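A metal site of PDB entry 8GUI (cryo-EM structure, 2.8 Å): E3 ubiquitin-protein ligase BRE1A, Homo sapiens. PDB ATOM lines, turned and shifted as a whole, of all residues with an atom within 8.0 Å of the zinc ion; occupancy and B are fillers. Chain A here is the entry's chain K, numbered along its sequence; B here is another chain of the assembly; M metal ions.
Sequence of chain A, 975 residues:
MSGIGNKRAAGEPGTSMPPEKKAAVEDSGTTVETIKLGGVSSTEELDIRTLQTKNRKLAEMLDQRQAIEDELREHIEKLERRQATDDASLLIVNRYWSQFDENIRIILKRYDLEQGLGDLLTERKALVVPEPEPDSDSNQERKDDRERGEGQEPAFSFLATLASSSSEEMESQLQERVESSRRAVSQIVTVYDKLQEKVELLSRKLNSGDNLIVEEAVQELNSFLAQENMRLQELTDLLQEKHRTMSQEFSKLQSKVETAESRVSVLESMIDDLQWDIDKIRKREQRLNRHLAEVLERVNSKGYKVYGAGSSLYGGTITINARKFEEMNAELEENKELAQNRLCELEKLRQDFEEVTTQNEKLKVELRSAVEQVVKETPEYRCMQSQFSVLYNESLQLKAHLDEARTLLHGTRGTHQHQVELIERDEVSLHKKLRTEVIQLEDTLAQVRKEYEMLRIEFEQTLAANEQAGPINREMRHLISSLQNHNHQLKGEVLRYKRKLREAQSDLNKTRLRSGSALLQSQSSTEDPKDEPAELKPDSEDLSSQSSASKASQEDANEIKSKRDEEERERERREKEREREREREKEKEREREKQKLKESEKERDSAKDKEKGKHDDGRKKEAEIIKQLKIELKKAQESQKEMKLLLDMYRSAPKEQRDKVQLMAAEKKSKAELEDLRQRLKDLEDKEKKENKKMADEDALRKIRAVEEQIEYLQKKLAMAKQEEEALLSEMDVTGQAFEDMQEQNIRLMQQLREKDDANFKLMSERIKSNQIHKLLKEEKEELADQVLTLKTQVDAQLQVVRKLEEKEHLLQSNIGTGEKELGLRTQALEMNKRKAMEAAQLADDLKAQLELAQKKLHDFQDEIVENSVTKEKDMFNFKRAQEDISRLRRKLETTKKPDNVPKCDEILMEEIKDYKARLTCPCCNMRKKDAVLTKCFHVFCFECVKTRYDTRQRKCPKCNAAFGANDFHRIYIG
Of the 17 residues printed, 4 come within 4 Å of the zinc ion.
ND1 of His 939 binds the zinc ion, at 2.1 Å.
The zinc ion is bound by SG of Cys 960 (2.3 Å).
SG of Cys 957 binds the zinc ion (2.3 Å).
SG of Cys 937 binds the zinc ion, 2.3 Å away.
O of His 939 lies within hydrogen-bond range of N of Leu 934 (2.9 Å).
The backbone carbonyl oxygen (O) of Ala 962 sits at hydrogen-bond distance from the backbone NH (N) of Cys 957.
The backbone carbonyl oxygen (O) of Cys 957 sits close to the side-chain amide oxygen (OD1) of Asn 961, 3.2 Å away.
The side-chain sulfur (SG) of Cys 960 lies close to the backbone NH (N) of Ala 962 (3.7 Å).
NZ of Lys 959 lies close to ND1 of His 939 (3.1 Å).
The backbone NH of Lys 959 sits close to the side-chain sulfur of Cys 957 (3.5 Å).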
ATOM      1  N   LEU A 934       0.174 -27.673   6.077  1.00  0.00           N
ATOM      2  CA  LEU A 934       0.256 -27.757   4.628  1.00  0.00           C
ATOM      3  C   LEU A 934       0.111 -29.212   4.190  1.00  0.00           C
ATOM      4  O   LEU A 934       0.637 -30.122   4.846  1.00  0.00           O
ATOM      5  CB  LEU A 934       1.577 -27.186   4.113  1.00  0.00           C
ATOM      6  CG  LEU A 934       2.024 -25.828   4.664  1.00  0.00           C
ATOM      7  CD1 LEU A 934       3.271 -25.354   3.951  1.00  0.00           C
ATOM      8  CD2 LEU A 934       0.923 -24.807   4.544  1.00  0.00           C
ATOM      9  N   LYS A 936       1.093 -30.371   1.110  1.00  0.00           N
ATOM     10  CA  LYS A 936       2.156 -30.786   0.195  1.00  0.00           C
ATOM     11  C   LYS A 936       3.379 -31.291   0.954  1.00  0.00           C
ATOM     12  O   LYS A 936       3.757 -32.458   0.839  1.00  0.00           O
ATOM     13  CB  LYS A 936       2.521 -29.629  -0.730  1.00  0.00           C
ATOM     14  CG  LYS A 936       1.384 -29.158  -1.619  1.00  0.00           C
ATOM     15  CD  LYS A 936       0.913 -30.267  -2.541  1.00  0.00           C
ATOM     16  CE  LYS A 936       1.979 -30.619  -3.563  1.00  0.00           C
ATOM     17  NZ  LYS A 936       2.258 -29.483  -4.486  1.00  0.00           N
ATOM     18  N   CYS A 937       3.996 -30.423   1.741  1.00  0.00           N
ATOM     19  CA  CYS A 937       5.187 -30.792   2.502  1.00  0.00           C
ATOM     20  C   CYS A 937       4.854 -31.400   3.855  1.00  0.00           C
ATOM     21  O   CYS A 937       5.764 -31.873   4.547  1.00  0.00           O
ATOM     22  CB  CYS A 937       6.096 -29.577   2.691  1.00  0.00           C
ATOM     23  SG  CYS A 937       5.388 -28.265   3.713  1.00  0.00           S
ATOM     24  N   PHE A 938       3.578 -31.389   4.245  1.00  0.00           N
ATOM     25  CA  PHE A 938       3.104 -31.967   5.499  1.00  0.00           C
ATOM     26  C   PHE A 938       3.840 -31.381   6.699  1.00  0.00           C
ATOM     27  O   PHE A 938       4.296 -32.104   7.598  1.00  0.00           O
ATOM     28  CB  PHE A 938       3.190 -33.493   5.467  1.00  0.00           C
ATOM     29  CG  PHE A 938       2.049 -34.140   4.750  1.00  0.00           C
ATOM     30  CD1 PHE A 938       0.765 -34.077   5.274  1.00  0.00           C
ATOM     31  CD2 PHE A 938       2.255 -34.811   3.548  1.00  0.00           C
ATOM     32  CE1 PHE A 938      -0.294 -34.667   4.611  1.00  0.00           C
ATOM     33  CE2 PHE A 938       1.196 -35.402   2.884  1.00  0.00           C
ATOM     34  CZ  PHE A 938      -0.082 -35.331   3.419  1.00  0.00           C
ATOM     35  N   HIS A 939       3.957 -30.067   6.706  1.00  0.00           N
ATOM     36  CA  HIS A 939       4.496 -29.321   7.827  1.00  0.00           C
ATOM     37  C   HIS A 939       3.394 -28.465   8.458  1.00  0.00           C
ATOM     38  O   HIS A 939       2.311 -28.302   7.894  1.00  0.00           O
ATOM     39  CB  HIS A 939       5.677 -28.441   7.395  1.00  0.00           C
ATOM     40  CG  HIS A 939       6.801 -29.219   6.782  1.00  0.00           C
ATOM     41  ND1 HIS A 939       7.622 -28.696   5.806  1.00  0.00           N
ATOM     42  CD2 HIS A 939       7.237 -30.487   6.996  1.00  0.00           C
ATOM     43  CE1 HIS A 939       8.513 -29.593   5.450  1.00  0.00           C
ATOM     44  NE2 HIS A 939       8.300 -30.695   6.159  1.00  0.00           N
ATOM     45  N   VAL A 940       3.690 -27.934   9.635  1.00  0.00           N
ATOM     46  CA  VAL A 940       2.697 -27.251  10.459  1.00  0.00           C
ATOM     47  C   VAL A 940       3.162 -25.817  10.686  1.00  0.00           C
ATOM     48  O   VAL A 940       4.319 -25.573  11.045  1.00  0.00           O
ATOM     49  CB  VAL A 940       2.489 -27.981  11.800  1.00  0.00           C
ATOM     50  CG1 VAL A 940       1.543 -27.204  12.693  1.00  0.00           C
ATOM     51  CG2 VAL A 940       1.977 -29.389  11.554  1.00  0.00           C
ATOM     52  N   PHE A 941       2.258 -24.869  10.463  1.00  0.00           N
ATOM     53  CA  PHE A 941       2.510 -23.443  10.686  1.00  0.00           C
ATOM     54  C   PHE A 941       1.273 -22.851  11.329  1.00  0.00           C
ATOM     55  O   PHE A 941       0.390 -23.572  11.818  1.00  0.00           O
ATOM     56  CB  PHE A 941       2.878 -22.743   9.371  1.00  0.00           C
ATOM     57  CG  PHE A 941       4.131 -23.273   8.732  1.00  0.00           C
ATOM     58  CD1 PHE A 941       4.074 -24.300   7.810  1.00  0.00           C
ATOM     59  CD2 PHE A 941       5.363 -22.724   9.049  1.00  0.00           C
ATOM     60  CE1 PHE A 941       5.225 -24.782   7.222  1.00  0.00           C
ATOM     61  CE2 PHE A 941       6.514 -23.207   8.461  1.00  0.00           C
ATOM     62  CZ  PHE A 941       6.449 -24.235   7.544  1.00  0.00           C
ATOM     63  N   LYS A 956       4.821 -20.612  -1.158  1.00  0.00           N
ATOM     64  CA  LYS A 956       5.779 -21.684  -0.939  1.00  0.00           C
ATOM     65  C   LYS A 956       5.963 -21.858   0.564  1.00  0.00           C
ATOM     66  O   LYS A 956       5.701 -20.947   1.352  1.00  0.00           O
ATOM     67  CB  LYS A 956       7.126 -21.398  -1.619  1.00  0.00           C
ATOM     68  CG  LYS A 956       7.078 -21.431  -3.130  1.00  0.00           C
ATOM     69  CD  LYS A 956       8.416 -21.030  -3.739  1.00  0.00           C
ATOM     70  CE  LYS A 956       8.355 -21.030  -5.256  1.00  0.00           C
ATOM     71  NZ  LYS A 956       7.447 -19.973  -5.771  1.00  0.00           N
ATOM     72  N   CYS A 957       6.417 -23.043   0.953  1.00  0.00           N
ATOM     73  CA  CYS A 957       6.670 -23.305   2.368  1.00  0.00           C
ATOM     74  C   CYS A 957       7.818 -22.422   2.860  1.00  0.00           C
ATOM     75  O   CYS A 957       8.784 -22.213   2.127  1.00  0.00           O
ATOM     76  CB  CYS A 957       6.985 -24.771   2.616  1.00  0.00           C
ATOM     77  SG  CYS A 957       7.434 -25.141   4.318  1.00  0.00           S
ATOM     78  N   PRO A 958       7.722 -21.881   4.076  1.00  0.00           N
ATOM     79  CA  PRO A 958       8.792 -21.022   4.577  1.00  0.00           C
ATOM     80  C   PRO A 958      10.159 -21.689   4.662  1.00  0.00           C
ATOM     81  O   PRO A 958      11.173 -20.987   4.615  1.00  0.00           O
ATOM     82  CB  PRO A 958       8.283 -20.604   5.960  1.00  0.00           C
ATOM     83  CG  PRO A 958       6.809 -20.656   5.834  1.00  0.00           C
ATOM     84  CD  PRO A 958       6.514 -21.810   4.920  1.00  0.00           C
ATOM     85  N   LYS A 959      10.223 -23.018   4.806  1.00  0.00           N
ATOM     86  CA  LYS A 959      11.515 -23.684   4.959  1.00  0.00           C
ATOM     87  C   LYS A 959      11.873 -24.623   3.815  1.00  0.00           C
ATOM     88  O   LYS A 959      13.012 -24.613   3.360  1.00  0.00           O
ATOM     89  CB  LYS A 959      11.569 -24.427   6.310  1.00  0.00           C
ATOM     90  CG  LYS A 959      10.598 -25.570   6.501  1.00  0.00           C
ATOM     91  CD  LYS A 959      10.753 -26.149   7.894  1.00  0.00           C
ATOM     92  CE  LYS A 959       9.820 -27.318   8.140  1.00  0.00           C
ATOM     93  NZ  LYS A 959       8.412 -26.839   8.158  1.00  0.00           N
ATOM     94  N   CYS A 960      10.939 -25.441   3.314  1.00  0.00           N
ATOM     95  CA  CYS A 960      11.281 -26.330   2.213  1.00  0.00           C
ATOM     96  C   CYS A 960      10.940 -25.749   0.850  1.00  0.00           C
ATOM     97  O   CYS A 960      11.254 -26.361  -0.170  1.00  0.00           O
ATOM     98  CB  CYS A 960      10.599 -27.698   2.352  1.00  0.00           C
ATOM     99  SG  CYS A 960       8.806 -27.682   2.243  1.00  0.00           S
ATOM    100  N   ASN A 961      10.297 -24.579   0.820  1.00  0.00           N
ATOM    101  CA  ASN A 961       9.950 -23.869  -0.416  1.00  0.00           C
ATOM    102  C   ASN A 961       9.075 -24.713  -1.349  1.00  0.00           C
ATOM    103  O   ASN A 961       9.159 -24.593  -2.573  1.00  0.00           O
ATOM    104  CB  ASN A 961      11.206 -23.389  -1.148  1.00  0.00           C
ATOM    105  CG  ASN A 961      11.564 -21.956  -0.812  1.00  0.00           C
ATOM    106  OD1 ASN A 961      11.318 -21.487   0.296  1.00  0.00           O
ATOM    107  ND2 ASN A 961      12.134 -21.255  -1.784  1.00  0.00           N
ATOM    108  N   ALA A 962       8.232 -25.566  -0.770  1.00  0.00           N
ATOM    109  CA  ALA A 962       7.321 -26.374  -1.577  1.00  0.00           C
ATOM    110  C   ALA A 962       6.082 -25.556  -1.924  1.00  0.00           C
ATOM    111  O   ALA A 962       5.429 -24.986  -1.041  1.00  0.00           O
ATOM    112  CB  ALA A 962       6.923 -27.637  -0.820  1.00  0.00           C
ATOM    113  N   ALA A 963       5.759 -25.498  -3.215  1.00  0.00           N
ATOM    114  CA  ALA A 963       4.604 -24.731  -3.667  1.00  0.00           C
ATOM    115  C   ALA A 963       3.323 -25.423  -3.238  1.00  0.00           C
ATOM    116  O   ALA A 963       3.165 -26.640  -3.427  1.00  0.00           O
ATOM    117  CB  ALA A 963       4.648 -24.564  -5.184  1.00  0.00           C
ATOM    118  N   PHE A 964       2.406 -24.654  -2.664  1.00  0.00           N
ATOM    119  CA  PHE A 964       1.144 -25.189  -2.163  1.00  0.00           C
ATOM    120  C   PHE A 964      -0.016 -24.355  -2.700  1.00  0.00           C
ATOM    121  O   PHE A 964       0.115 -23.147  -2.931  1.00  0.00           O
ATOM    122  CB  PHE A 964       1.118 -25.205  -0.629  1.00  0.00           C
ATOM    123  CG  PHE A 964       1.239 -23.851   0.006  1.00  0.00           C
ATOM    124  CD1 PHE A 964       2.477 -23.287   0.238  1.00  0.00           C
ATOM    125  CD2 PHE A 964       0.101 -23.149   0.387  1.00  0.00           C
ATOM    126  CE1 PHE A 964       2.586 -22.043   0.823  1.00  0.00           C
ATOM    127  CE2 PHE A 964       0.210 -21.905   0.972  1.00  0.00           C
ATOM    128  CZ  PHE A 964       1.455 -21.349   1.195  1.00  0.00           C
ATOM    129  N   TYR B 999       4.564 -33.058  10.539  1.00  0.00           N
ATOM    130  CA  TYR B 999       5.823 -32.693  11.187  1.00  0.00           C
ATOM    131  C   TYR B 999       5.521 -31.601  12.205  1.00  0.00           C
ATOM    132  O   TYR B 999       5.221 -30.462  11.829  1.00  0.00           O
ATOM    133  CB  TYR B 999       6.839 -32.233  10.141  1.00  0.00           C
ATOM    134  CG  TYR B 999       8.222 -31.887  10.645  1.00  0.00           C
ATOM    135  CD1 TYR B 999       8.639 -32.264  11.920  1.00  0.00           C
ATOM    136  CD2 TYR B 999       9.120 -31.188   9.846  1.00  0.00           C
ATOM    137  CE1 TYR B 999       9.911 -31.946  12.377  1.00  0.00           C
ATOM    138  CE2 TYR B 999      10.386 -30.877  10.294  1.00  0.00           C
ATOM    139  CZ  TYR B 999      10.775 -31.249  11.553  1.00  0.00           C
ATOM    140  OH  TYR B 999      12.041 -30.938  12.000  1.00  0.00           O
HETATM  141 ZN    ZN M   1       7.524 -27.452   4.152  1.00  0.00          ZN
